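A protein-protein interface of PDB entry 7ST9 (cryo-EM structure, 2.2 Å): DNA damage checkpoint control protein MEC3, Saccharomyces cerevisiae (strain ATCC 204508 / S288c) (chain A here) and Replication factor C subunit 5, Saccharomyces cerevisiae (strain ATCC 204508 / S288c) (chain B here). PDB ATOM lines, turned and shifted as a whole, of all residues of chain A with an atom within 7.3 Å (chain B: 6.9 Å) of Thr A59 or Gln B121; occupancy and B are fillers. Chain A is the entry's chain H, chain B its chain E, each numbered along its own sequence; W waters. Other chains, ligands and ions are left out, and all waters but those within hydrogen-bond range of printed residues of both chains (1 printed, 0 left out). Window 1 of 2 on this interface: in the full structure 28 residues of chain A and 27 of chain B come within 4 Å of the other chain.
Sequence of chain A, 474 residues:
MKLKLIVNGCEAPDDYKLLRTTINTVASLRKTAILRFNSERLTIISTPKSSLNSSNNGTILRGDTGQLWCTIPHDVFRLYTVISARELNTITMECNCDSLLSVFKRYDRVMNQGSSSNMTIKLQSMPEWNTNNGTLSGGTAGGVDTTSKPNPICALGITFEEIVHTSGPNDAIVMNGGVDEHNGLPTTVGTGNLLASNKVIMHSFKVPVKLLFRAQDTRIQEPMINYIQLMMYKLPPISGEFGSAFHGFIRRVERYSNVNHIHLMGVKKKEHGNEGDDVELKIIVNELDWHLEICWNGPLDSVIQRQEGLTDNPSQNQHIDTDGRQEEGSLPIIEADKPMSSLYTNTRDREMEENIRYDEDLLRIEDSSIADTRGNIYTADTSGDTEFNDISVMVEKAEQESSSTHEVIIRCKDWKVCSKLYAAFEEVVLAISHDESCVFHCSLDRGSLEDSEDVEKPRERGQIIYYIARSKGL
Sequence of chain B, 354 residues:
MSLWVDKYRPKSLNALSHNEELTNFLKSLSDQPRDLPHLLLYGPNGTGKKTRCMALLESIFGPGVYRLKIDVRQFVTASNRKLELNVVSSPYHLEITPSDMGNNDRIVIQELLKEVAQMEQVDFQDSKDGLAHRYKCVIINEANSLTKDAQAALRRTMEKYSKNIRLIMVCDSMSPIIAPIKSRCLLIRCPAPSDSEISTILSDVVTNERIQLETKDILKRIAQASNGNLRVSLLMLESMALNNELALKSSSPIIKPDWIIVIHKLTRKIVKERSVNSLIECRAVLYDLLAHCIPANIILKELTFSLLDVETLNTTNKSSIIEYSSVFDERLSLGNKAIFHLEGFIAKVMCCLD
Water W1 lies within hydrogen-bond range of NZ of Lys B136 (2.9 Å) and O of Thr A59 (3.1 Å).
Of the 17 printed residues of chain B, 12 touch a printed residue of chain A. Of the 18 printed residues of chain A, 11 touch a printed residue of chain B. Along chain A the printed residues that touch a printed residue of chain B span positions 49 to 395.
Thr A59 touches one residue of chain B. Gln B121 touches two residues of chain A. No residue of chain B comes within 4 Å of Gly A58. Of the printed residues of chain A, Lys B136 touches Ile A60. Printed residues of chain B within 4 Å of Gly A63: Met B119. Of the printed residues of chain B, Arg A62 touches Met B119. Of the printed residues of chain A, Ala B132 touches Val A393. Of the printed residues of chain B, Ile A60 touches Pro B91 (3.8 Å), Tyr B92 (3.3 Å), Gln B121 (3.6 Å) and Lys B136 (3.8 Å). The nearest residue of chain B that does not touch Thr A59 is Val B122 (4.4 Å). The nearest printed residue of chain A that does not touch Asp B123 is Pro A48 (4.9 Å).
Among the printed residues, merely in contact across the chains: Ile A60 with Tyr B92 (3.3 Å), Val A393 with Ala B132 (3.3 Å), Leu A61 with Met B119 (3.4 Å), Val A395 with Val B122 (3.5 Å), Asn A57 with Pro B91 (3.5 Å), Ile A391 with Arg B134 (3.6 Å), Ile A60 with Gln B121 (3.6 Å), Ile A391 with Tyr B135 (3.6 Å), Ile A391 with His B133 (3.7 Å), Thr A65 with Asp B123 (3.8 Å), Ile A60 with Lys B136 (3.8 Å), Ile A391 with Phe B61 (3.8 Å), Ile A60 with Pro B91 (3.8 Å), Val A395 with His B133 (3.8 Å), Gly A63 with Met B119 (3.9 Å), Arg A62 with Met B119 (3.9 Å) and Thr A59 with Gln B121 (3.9 Å).
O of Val B122 lies within hydrogen-bond range of OG1 of Thr A65 (3.0 Å). The side-chain carboxylate (OD2) of Asp B123 is in salt-bridge range of the side-chain amino group (NZ) of Lys A49, 2.9 Å away. O of Val A393 lies within hydrogen-bond range of N of His B133.
NZ of Lys B136 sits at hydrogen-bond distance from O of Met B119 (2.8 Å). The backbone carbonyl oxygen of Asp B123 lies within hydrogen-bond range of the backbone NH of Ala B132 (2.9 Å). OD2 of Asp B123 lies within salt-bridge range of NH2 of Arg B134 (3.99 Å). O of Lys A49 lies within hydrogen-bond range of OG of Ser A54 (3.2 Å). The side-chain amide oxygen (OD1) of Asn A57 sits close to the backbone carbonyl oxygen (O) of Ser A54 (2.8 Å). N of Gly A63 is in hydrogen-bond range of O of Gly A58 (3.2 Å).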
ATOM      1  N   ARG A  30       5.292 -25.701   2.824  1.00  0.00           N
ATOM      2  CA  ARG A  30       6.661 -25.489   3.276  1.00  0.00           C
ATOM      3  C   ARG A  30       7.132 -26.730   4.022  1.00  0.00           C
ATOM      4  O   ARG A  30       6.339 -27.597   4.394  1.00  0.00           O
ATOM      5  CB  ARG A  30       6.769 -24.238   4.153  1.00  0.00           C
ATOM      6  CG  ARG A  30       7.460 -23.069   3.466  1.00  0.00           C
ATOM      7  CD  ARG A  30       7.369 -21.794   4.288  1.00  0.00           C
ATOM      8  NE  ARG A  30       5.989 -21.372   4.500  1.00  0.00           N
ATOM      9  CZ  ARG A  30       5.321 -20.543   3.708  1.00  0.00           C
ATOM     10  NH1 ARG A  30       5.872 -20.025   2.622  1.00  0.00           N
ATOM     11  NH2 ARG A  30       4.066 -20.225   4.015  1.00  0.00           N
ATOM     12  N   PRO A  48       7.183 -18.004   6.021  1.00  0.00           N
ATOM     13  CA  PRO A  48       8.606 -18.011   5.643  1.00  0.00           C
ATOM     14  C   PRO A  48       9.525 -17.456   6.717  1.00  0.00           C
ATOM     15  O   PRO A  48      10.745 -17.642   6.616  1.00  0.00           O
ATOM     16  CB  PRO A  48       8.641 -17.142   4.379  1.00  0.00           C
ATOM     17  CG  PRO A  48       7.428 -16.284   4.472  1.00  0.00           C
ATOM     18  CD  PRO A  48       6.390 -17.128   5.141  1.00  0.00           C
ATOM     19  N   LYS A  49       8.987 -16.789   7.734  1.00  0.00           N
ATOM     20  CA  LYS A  49       9.782 -16.176   8.787  1.00  0.00           C
ATOM     21  C   LYS A  49      10.193 -17.162   9.874  1.00  0.00           C
ATOM     22  O   LYS A  49      10.927 -16.779  10.791  1.00  0.00           O
ATOM     23  CB  LYS A  49       9.007 -15.015   9.418  1.00  0.00           C
ATOM     24  CG  LYS A  49       8.494 -13.999   8.409  1.00  0.00           C
ATOM     25  CD  LYS A  49       7.976 -12.745   9.093  1.00  0.00           C
ATOM     26  CE  LYS A  49       7.786 -11.607   8.102  1.00  0.00           C
ATOM     27  NZ  LYS A  49       6.659 -11.860   7.163  1.00  0.00           N
ATOM     28  N   ASN A  53      12.404 -22.288   8.175  1.00  0.00           N
ATOM     29  CA  ASN A  53      11.994 -21.914   6.826  1.00  0.00           C
ATOM     30  C   ASN A  53      12.860 -20.795   6.260  1.00  0.00           C
ATOM     31  O   ASN A  53      13.169 -20.794   5.063  1.00  0.00           O
ATOM     32  CB  ASN A  53      10.523 -21.496   6.824  1.00  0.00           C
ATOM     33  CG  ASN A  53       9.584 -22.670   7.014  1.00  0.00           C
ATOM     34  OD1 ASN A  53       9.853 -23.777   6.549  1.00  0.00           O
ATOM     35  ND2 ASN A  53       8.471 -22.432   7.700  1.00  0.00           N
ATOM     36  N   SER A  54      13.262 -19.837   7.098  1.00  0.00           N
ATOM     37  CA  SER A  54      14.055 -18.713   6.613  1.00  0.00           C
ATOM     38  C   SER A  54      15.399 -19.155   6.050  1.00  0.00           C
ATOM     39  O   SER A  54      15.998 -18.419   5.259  1.00  0.00           O
ATOM     40  CB  SER A  54      14.277 -17.698   7.737  1.00  0.00           C
ATOM     41  OG  SER A  54      13.135 -17.593   8.567  1.00  0.00           O
ATOM     42  N   ASN A  56      15.946 -21.539   3.916  1.00  0.00           N
ATOM     43  CA  ASN A  56      15.786 -21.803   2.490  1.00  0.00           C
ATOM     44  C   ASN A  56      15.799 -20.536   1.646  1.00  0.00           C
ATOM     45  O   ASN A  56      15.927 -20.635   0.421  1.00  0.00           O
ATOM     46  CB  ASN A  56      14.485 -22.567   2.244  1.00  0.00           C
ATOM     47  CG  ASN A  56      14.703 -24.060   2.102  1.00  0.00           C
ATOM     48  OD1 ASN A  56      14.324 -24.840   2.975  1.00  0.00           O
ATOM     49  ND2 ASN A  56      15.319 -24.464   0.996  1.00  0.00           N
ATOM     50  N   ASN A  57      15.664 -19.359   2.258  1.00  0.00           N
ATOM     51  CA  ASN A  57      15.709 -18.092   1.530  1.00  0.00           C
ATOM     52  C   ASN A  57      14.701 -18.082   0.382  1.00  0.00           C
ATOM     53  O   ASN A  57      14.992 -17.634  -0.727  1.00  0.00           O
ATOM     54  CB  ASN A  57      17.120 -17.810   1.012  1.00  0.00           C
ATOM     55  CG  ASN A  57      18.159 -17.819   2.116  1.00  0.00           C
ATOM     56  OD1 ASN A  57      17.837 -17.623   3.287  1.00  0.00           O
ATOM     57  ND2 ASN A  57      19.413 -18.048   1.746  1.00  0.00           N
ATOM     58  N   GLY A  58      13.498 -18.589   0.657  1.00  0.00           N
ATOM     59  CA  GLY A  58      12.469 -18.627  -0.367  1.00  0.00           C
ATOM     60  C   GLY A  58      11.996 -17.253  -0.796  1.00  0.00           C
ATOM     61  O   GLY A  58      11.679 -17.044  -1.970  1.00  0.00           O
ATOM     62  N   THR A  59      11.943 -16.301   0.137  1.00  0.00           N
ATOM     63  CA  THR A  59      11.389 -14.988  -0.176  1.00  0.00           C
ATOM     64  C   THR A  59      12.187 -14.289  -1.272  1.00  0.00           C
ATOM     65  O   THR A  59      11.607 -13.711  -2.198  1.00  0.00           O
ATOM     66  CB  THR A  59      11.349 -14.124   1.085  1.00  0.00           C
ATOM     67  OG1 THR A  59      10.603 -14.798   2.107  1.00  0.00           O
ATOM     68  CG2 THR A  59      10.704 -12.775   0.794  1.00  0.00           C
ATOM     69  N   ILE A  60      13.520 -14.333  -1.188  1.00  0.00           N
ATOM     70  CA  ILE A  60      14.354 -13.584  -2.126  1.00  0.00           C
ATOM     71  C   ILE A  60      14.601 -14.319  -3.433  1.00  0.00           C
ATOM     72  O   ILE A  60      15.039 -13.693  -4.405  1.00  0.00           O
ATOM     73  CB  ILE A  60      15.713 -13.238  -1.488  1.00  0.00           C
ATOM     74  CG1 ILE A  60      16.458 -12.212  -2.346  1.00  0.00           C
ATOM     75  CG2 ILE A  60      16.559 -14.492  -1.305  1.00  0.00           C
ATOM     76  CD1 ILE A  60      17.517 -11.441  -1.592  1.00  0.00           C
ATOM     77  N   LEU A  61      14.327 -15.622  -3.492  1.00  0.00           N
ATOM     78  CA  LEU A  61      14.612 -16.420  -4.678  1.00  0.00           C
ATOM     79  C   LEU A  61      13.376 -16.816  -5.468  1.00  0.00           C
ATOM     80  O   LEU A  61      13.458 -16.930  -6.693  1.00  0.00           O
ATOM     81  CB  LEU A  61      15.368 -17.696  -4.288  1.00  0.00           C
ATOM     82  CG  LEU A  61      16.874 -17.533  -4.090  1.00  0.00           C
ATOM     83  CD1 LEU A  61      17.411 -18.645  -3.211  1.00  0.00           C
ATOM     84  CD2 LEU A  61      17.597 -17.509  -5.429  1.00  0.00           C
ATOM     85  N   ARG A  62      12.239 -17.032  -4.806  1.00  0.00           N
ATOM     86  CA  ARG A  62      11.043 -17.511  -5.483  1.00  0.00           C
ATOM     87  C   ARG A  62       9.777 -16.778  -5.064  1.00  0.00           C
ATOM     88  O   ARG A  62       8.694 -17.151  -5.524  1.00  0.00           O
ATOM     89  CB  ARG A  62      10.867 -19.017  -5.227  1.00  0.00           C
ATOM     90  CG  ARG A  62      11.866 -19.890  -5.977  1.00  0.00           C
ATOM     91  CD  ARG A  62      12.383 -21.054  -5.133  1.00  0.00           C
ATOM     92  NE  ARG A  62      11.410 -21.520  -4.150  1.00  0.00           N
ATOM     93  CZ  ARG A  62      11.681 -21.801  -2.881  1.00  0.00           C
ATOM     94  NH1 ARG A  62      12.905 -21.691  -2.389  1.00  0.00           N
ATOM     95  NH2 ARG A  62      10.696 -22.206  -2.083  1.00  0.00           N
ATOM     96  N   GLY A  63       9.872 -15.758  -4.219  1.00  0.00           N
ATOM     97  CA  GLY A  63       8.699 -15.012  -3.797  1.00  0.00           C
ATOM     98  C   GLY A  63       7.721 -15.802  -2.954  1.00  0.00           C
ATOM     99  O   GLY A  63       6.505 -15.697  -3.163  1.00  0.00           O
ATOM    100  N   ASP A  64       8.218 -16.590  -2.002  1.00  0.00           N
ATOM    101  CA  ASP A  64       7.362 -17.363  -1.100  1.00  0.00           C
ATOM    102  C   ASP A  64       6.951 -16.463   0.057  1.00  0.00           C
ATOM    103  O   ASP A  64       7.573 -16.455   1.121  1.00  0.00           O
ATOM    104  CB  ASP A  64       8.082 -18.611  -0.606  1.00  0.00           C
ATOM    105  CG  ASP A  64       8.718 -19.399  -1.730  1.00  0.00           C
ATOM    106  OD1 ASP A  64       9.596 -18.843  -2.422  1.00  0.00           O
ATOM    107  OD2 ASP A  64       8.341 -20.574  -1.923  1.00  0.00           O
ATOM    108  N   THR A  65       5.883 -15.692  -0.154  1.00  0.00           N
ATOM    109  CA  THR A  65       5.397 -14.748   0.843  1.00  0.00           C
ATOM    110  C   THR A  65       4.099 -15.179   1.511  1.00  0.00           C
ATOM    111  O   THR A  65       3.773 -14.654   2.579  1.00  0.00           O
ATOM    112  CB  THR A  65       5.191 -13.366   0.204  1.00  0.00           C
ATOM    113  OG1 THR A  65       6.428 -12.901  -0.347  1.00  0.00           O
ATOM    114  CG2 THR A  65       4.692 -12.358   1.232  1.00  0.00           C
ATOM    115  N   ILE A 391      15.697  -0.638   4.689  1.00  0.00           N
ATOM    116  CA  ILE A 391      15.378  -0.191   3.340  1.00  0.00           C
ATOM    117  C   ILE A 391      13.933  -0.528   2.962  1.00  0.00           C
ATOM    118  O   ILE A 391      13.585  -0.520   1.783  1.00  0.00           O
ATOM    119  CB  ILE A 391      16.366  -0.767   2.312  1.00  0.00           C
ATOM    120  CG1 ILE A 391      16.435  -2.293   2.425  1.00  0.00           C
ATOM    121  CG2 ILE A 391      17.746  -0.165   2.511  1.00  0.00           C
ATOM    122  CD1 ILE A 391      16.368  -3.003   1.092  1.00  0.00           C
ATOM    123  N   VAL A 393      10.084  -0.116   2.200  1.00  0.00           N
ATOM    124  CA  VAL A 393       9.205   0.938   1.709  1.00  0.00           C
ATOM    125  C   VAL A 393       7.837   0.338   1.421  1.00  0.00           C
ATOM    126  O   VAL A 393       7.688  -0.871   1.230  1.00  0.00           O
ATOM    127  CB  VAL A 393       9.762   1.626   0.441  1.00  0.00           C
ATOM    128  CG1 VAL A 393      10.814   2.657   0.812  1.00  0.00           C
ATOM    129  CG2 VAL A 393      10.332   0.594  -0.519  1.00  0.00           C
ATOM    130  N   VAL A 395       4.650  -0.621  -0.700  1.00  0.00           N
ATOM    131  CA  VAL A 395       4.415  -0.976  -2.094  1.00  0.00           C
ATOM    132  C   VAL A 395       3.511   0.064  -2.739  1.00  0.00           C
ATOM    133  O   VAL A 395       2.591   0.599  -2.108  1.00  0.00           O
ATOM    134  CB  VAL A 395       3.804  -2.382  -2.197  1.00  0.00           C
ATOM    135  CG1 VAL A 395       4.734  -3.415  -1.579  1.00  0.00           C
ATOM    136  CG2 VAL A 395       2.432  -2.423  -1.534  1.00  0.00           C
ATOM    137  N   PHE B  61      21.712  -4.603   6.290  1.00  0.00           N
ATOM    138  CA  PHE B  61      20.729  -5.599   6.702  1.00  0.00           C
ATOM    139  C   PHE B  61      21.004  -6.196   8.073  1.00  0.00           C
ATOM    140  O   PHE B  61      20.113  -6.201   8.924  1.00  0.00           O
ATOM    141  CB  PHE B  61      20.669  -6.734   5.671  1.00  0.00           C
ATOM    142  CG  PHE B  61      20.208  -6.293   4.311  1.00  0.00           C
ATOM    143  CD1 PHE B  61      18.865  -6.072   4.057  1.00  0.00           C
ATOM    144  CD2 PHE B  61      21.120  -6.099   3.285  1.00  0.00           C
ATOM    145  CE1 PHE B  61      18.439  -5.667   2.806  1.00  0.00           C
ATOM    146  CE2 PHE B  61      20.699  -5.692   2.035  1.00  0.00           C
ATOM    147  CZ  PHE B  61      19.357  -5.476   1.795  1.00  0.00           C
ATOM    148  N   PRO B  91      19.557 -14.557   2.913  1.00  0.00           N
ATOM    149  CA  PRO B  91      18.182 -14.038   2.986  1.00  0.00           C
ATOM    150  C   PRO B  91      18.025 -12.636   2.423  1.00  0.00           C
ATOM    151  O   PRO B  91      16.897 -12.245   2.094  1.00  0.00           O
ATOM    152  CB  PRO B  91      17.866 -14.077   4.490  1.00  0.00           C
ATOM    153  CG  PRO B  91      19.183 -14.223   5.176  1.00  0.00           C
ATOM    154  CD  PRO B  91      20.071 -14.957   4.233  1.00  0.00           C
ATOM    155  N   TYR B  92      19.108 -11.864   2.301  1.00  0.00           N
ATOM    156  CA  TYR B  92      19.024 -10.488   1.832  1.00  0.00           C
ATOM    157  C   TYR B  92      19.733 -10.226   0.511  1.00  0.00           C
ATOM    158  O   TYR B  92      19.476  -9.185  -0.104  1.00  0.00           O
ATOM    159  CB  TYR B  92      19.593  -9.526   2.887  1.00  0.00           C
ATOM    160  CG  TYR B  92      19.223  -9.873   4.311  1.00  0.00           C
ATOM    161  CD1 TYR B  92      17.992  -9.503   4.838  1.00  0.00           C
ATOM    162  CD2 TYR B  92      20.108 -10.557   5.133  1.00  0.00           C
ATOM    163  CE1 TYR B  92      17.651  -9.812   6.141  1.00  0.00           C
ATOM    164  CE2 TYR B  92      19.775 -10.870   6.437  1.00  0.00           C
ATOM    165  CZ  TYR B  92      18.546 -10.496   6.935  1.00  0.00           C
ATOM    166  OH  TYR B  92      18.212 -10.807   8.234  1.00  0.00           O
ATOM    167  N   VAL B 116      15.446 -12.075 -11.691  1.00  0.00           N
ATOM    168  CA  VAL B 116      15.618 -11.553 -10.340  1.00  0.00           C
ATOM    169  C   VAL B 116      15.245 -10.080 -10.300  1.00  0.00           C
ATOM    170  O   VAL B 116      14.636  -9.601  -9.337  1.00  0.00           O
ATOM    171  CB  VAL B 116      17.062 -11.786  -9.855  1.00  0.00           C
ATOM    172  CG1 VAL B 116      17.317 -11.035  -8.555  1.00  0.00           C
ATOM    173  CG2 VAL B 116      17.333 -13.271  -9.681  1.00  0.00           C
ATOM    174  N   GLN B 118      13.085  -8.645 -12.273  1.00  0.00           N
ATOM    175  CA  GLN B 118      11.674  -8.451 -12.585  1.00  0.00           C
ATOM    176  C   GLN B 118      10.766  -8.815 -11.417  1.00  0.00           C
ATOM    177  O   GLN B 118       9.687  -8.229 -11.274  1.00  0.00           O
ATOM    178  CB  GLN B 118      11.295  -9.274 -13.818  1.00  0.00           C
ATOM    179  CG  GLN B 118      11.631  -8.592 -15.135  1.00  0.00           C
ATOM    180  CD  GLN B 118      11.462  -9.511 -16.329  1.00  0.00           C
ATOM    181  OE1 GLN B 118      11.268 -10.716 -16.177  1.00  0.00           O
ATOM    182  NE2 GLN B 118      11.537  -8.942 -17.526  1.00  0.00           N
ATOM    183  N   MET B 119      11.176  -9.762 -10.579  1.00  0.00           N
ATOM    184  CA  MET B 119      10.350 -10.221  -9.465  1.00  0.00           C
ATOM    185  C   MET B 119      10.535  -9.267  -8.293  1.00  0.00           C
ATOM    186  O   MET B 119      11.556  -9.298  -7.605  1.00  0.00           O
ATOM    187  CB  MET B 119      10.721 -11.648  -9.080  1.00  0.00           C
ATOM    188  CG  MET B 119       9.644 -12.377  -8.292  1.00  0.00           C
ATOM    189  SD  MET B 119       9.977 -14.141  -8.127  1.00  0.00           S
ATOM    190  CE  MET B 119      11.550 -14.116  -7.274  1.00  0.00           C
ATOM    191  N   GLU B 120       9.542  -8.412  -8.063  1.00  0.00           N
ATOM    192  CA  GLU B 120       9.599  -7.486  -6.942  1.00  0.00           C
ATOM    193  C   GLU B 120       9.491  -8.244  -5.625  1.00  0.00           C
ATOM    194  O   GLU B 120       8.688  -9.171  -5.487  1.00  0.00           O
ATOM    195  CB  GLU B 120       8.477  -6.453  -7.049  1.00  0.00           C
ATOM    196  CG  GLU B 120       8.572  -5.321  -6.037  1.00  0.00           C
ATOM    197  CD  GLU B 120       7.278  -4.543  -5.907  1.00  0.00           C
ATOM    198  OE1 GLU B 120       6.279  -5.125  -5.434  1.00  0.00           O
ATOM    199  OE2 GLU B 120       7.258  -3.350  -6.275  1.00  0.00           O
ATOM    200  N   GLN B 121      10.312  -7.849  -4.656  1.00  0.00           N
ATOM    201  CA  GLN B 121      10.322  -8.479  -3.343  1.00  0.00           C
ATOM    202  C   GLN B 121       9.360  -7.737  -2.424  1.00  0.00           C
ATOM    203  O   GLN B 121       9.578  -6.563  -2.104  1.00  0.00           O
ATOM    204  CB  GLN B 121      11.733  -8.480  -2.756  1.00  0.00           C
ATOM    205  CG  GLN B 121      11.879  -9.322  -1.498  1.00  0.00           C
ATOM    206  CD  GLN B 121      13.300  -9.348  -0.973  1.00  0.00           C
ATOM    207  OE1 GLN B 121      14.051  -8.384  -1.129  1.00  0.00           O
ATOM    208  NE2 GLN B 121      13.680 -10.455  -0.346  1.00  0.00           N
ATOM    209  N   VAL B 122       8.299  -8.420  -2.002  1.00  0.00           N
ATOM    210  CA  VAL B 122       7.305  -7.858  -1.098  1.00  0.00           C
ATOM    211  C   VAL B 122       7.089  -8.831   0.050  1.00  0.00           C
ATOM    212  O   VAL B 122       7.309 -10.039  -0.082  1.00  0.00           O
ATOM    213  CB  VAL B 122       5.971  -7.559  -1.817  1.00  0.00           C
ATOM    214  CG1 VAL B 122       6.144  -6.413  -2.798  1.00  0.00           C
ATOM    215  CG2 VAL B 122       5.452  -8.803  -2.528  1.00  0.00           C
ATOM    216  N   ASP B 123       6.657  -8.295   1.189  1.00  0.00           N
ATOM    217  CA  ASP B 123       6.432  -9.114   2.371  1.00  0.00           C
ATOM    218  C   ASP B 123       5.376  -8.459   3.249  1.00  0.00           C
ATOM    219  O   ASP B 123       5.247  -7.233   3.283  1.00  0.00           O
ATOM    220  CB  ASP B 123       7.730  -9.316   3.163  1.00  0.00           C
ATOM    221  CG  ASP B 123       7.579 -10.330   4.279  1.00  0.00           C
ATOM    222  OD1 ASP B 123       7.038 -11.427   4.021  1.00  0.00           O
ATOM    223  OD2 ASP B 123       8.001 -10.032   5.417  1.00  0.00           O
ATOM    224  N   ALA B 132       5.280  -4.469   2.431  1.00  0.00           N
ATOM    225  CA  ALA B 132       6.522  -3.713   2.432  1.00  0.00           C
ATOM    226  C   ALA B 132       7.448  -4.297   1.376  1.00  0.00           C
ATOM    227  O   ALA B 132       7.540  -5.520   1.228  1.00  0.00           O
ATOM    228  CB  ALA B 132       7.199  -3.747   3.806  1.00  0.00           C
ATOM    229  N   HIS B 133       8.130  -3.419   0.645  1.00  0.00           N
ATOM    230  CA  HIS B 133       8.998  -3.809  -0.456  1.00  0.00           C
ATOM    231  C   HIS B 133      10.440  -3.441  -0.136  1.00  0.00           C
ATOM    232  O   HIS B 133      10.708  -2.385   0.445  1.00  0.00           O
ATOM    233  CB  HIS B 133       8.562  -3.135  -1.761  1.00  0.00           C
ATOM    234  CG  HIS B 133       9.675  -2.944  -2.743  1.00  0.00           C
ATOM    235  ND1 HIS B 133      10.271  -1.721  -2.965  1.00  0.00           N
ATOM    236  CD2 HIS B 133      10.299  -3.820  -3.567  1.00  0.00           C
ATOM    237  CE1 HIS B 133      11.215  -1.854  -3.879  1.00  0.00           C
ATOM    238  NE2 HIS B 133      11.251  -3.117  -4.261  1.00  0.00           N
ATOM    239  N   ARG B 134      11.363  -4.322  -0.517  1.00  0.00           N
ATOM    240  CA  ARG B 134      12.790  -4.098  -0.332  1.00  0.00           C
ATOM    241  C   ARG B 134      13.524  -4.530  -1.590  1.00  0.00           C
ATOM    242  O   ARG B 134      13.207  -5.571  -2.173  1.00  0.00           O
ATOM    243  CB  ARG B 134      13.325  -4.876   0.876  1.00  0.00           C
ATOM    244  CG  ARG B 134      13.112  -4.179   2.209  1.00  0.00           C
ATOM    245  CD  ARG B 134      13.454  -5.096   3.373  1.00  0.00           C
ATOM    246  NE  ARG B 134      12.520  -6.211   3.483  1.00  0.00           N
ATOM    247  CZ  ARG B 134      11.422  -6.207   4.227  1.00  0.00           C
ATOM    248  NH1 ARG B 134      11.073  -5.150   4.945  1.00  0.00           N
ATOM    249  NH2 ARG B 134      10.650  -7.290   4.251  1.00  0.00           N
ATOM    250  N   TYR B 135      14.503  -3.733  -2.010  1.00  0.00           N
ATOM    251  CA  TYR B 135      15.288  -4.097  -3.181  1.00  0.00           C
ATOM    252  C   TYR B 135      16.244  -5.237  -2.849  1.00  0.00           C
ATOM    253  O   TYR B 135      16.735  -5.362  -1.724  1.00  0.00           O
ATOM    254  CB  TYR B 135      16.059  -2.887  -3.720  1.00  0.00           C
ATOM    255  CG  TYR B 135      17.113  -2.306  -2.796  1.00  0.00           C
ATOM    256  CD1 TYR B 135      18.303  -2.981  -2.544  1.00  0.00           C
ATOM    257  CD2 TYR B 135      16.929  -1.066  -2.200  1.00  0.00           C
ATOM    258  CE1 TYR B 135      19.265  -2.446  -1.709  1.00  0.00           C
ATOM    259  CE2 TYR B 135      17.887  -0.522  -1.366  1.00  0.00           C
ATOM    260  CZ  TYR B 135      19.053  -1.216  -1.126  1.00  0.00           C
ATOM    261  OH  TYR B 135      20.008  -0.677  -0.296  1.00  0.00           O
ATOM    262  N   LYS B 136      16.498  -6.080  -3.845  1.00  0.00           N
ATOM    263  CA  LYS B 136      17.431  -7.188  -3.704  1.00  0.00           C
ATOM    264  C   LYS B 136      18.837  -6.738  -4.077  1.00  0.00           C
ATOM    265  O   LYS B 136      19.028  -5.996  -5.044  1.00  0.00           O
ATOM    266  CB  LYS B 136      17.019  -8.365  -4.592  1.00  0.00           C
ATOM    267  CG  LYS B 136      15.550  -8.737  -4.517  1.00  0.00           C
ATOM    268  CD  LYS B 136      15.219  -9.817  -5.533  1.00  0.00           C
ATOM    269  CE  LYS B 136      13.732 -10.108  -5.579  1.00  0.00           C
ATOM    270  NZ  LYS B 136      13.400 -11.120  -6.616  1.00  0.00           N
ATOM    271  N   CYS B 137      19.818  -7.195  -3.307  1.00  0.00           N
ATOM    272  CA  CYS B 137      21.222  -6.934  -3.589  1.00  0.00           C
ATOM    273  C   CYS B 137      21.815  -8.135  -4.312  1.00  0.00           C
ATOM    274  O   CYS B 137      21.580  -9.281  -3.917  1.00  0.00           O
ATOM    275  CB  CYS B 137      21.995  -6.650  -2.302  1.00  0.00           C
ATOM    276  SG  CYS B 137      21.762  -4.978  -1.659  1.00  0.00           S
ATOM    277  N   ASN B 164      13.910  -2.617  -7.851  1.00  0.00           N
ATOM    278  CA  ASN B 164      13.910  -3.961  -7.293  1.00  0.00           C
ATOM    279  C   ASN B 164      15.300  -4.559  -7.109  1.00  0.00           C
ATOM    280  O   ASN B 164      15.414  -5.618  -6.482  1.00  0.00           O
ATOM    281  CB  ASN B 164      13.089  -4.900  -8.187  1.00  0.00           C
ATOM    282  CG  ASN B 164      11.720  -4.342  -8.523  1.00  0.00           C
ATOM    283  OD1 ASN B 164      11.273  -3.360  -7.931  1.00  0.00           O
ATOM    284  ND2 ASN B 164      11.047  -4.967  -9.481  1.00  0.00           N
HETATM  285  O   HOH W   1      11.387 -11.870  -4.674  1.00  0.00           O
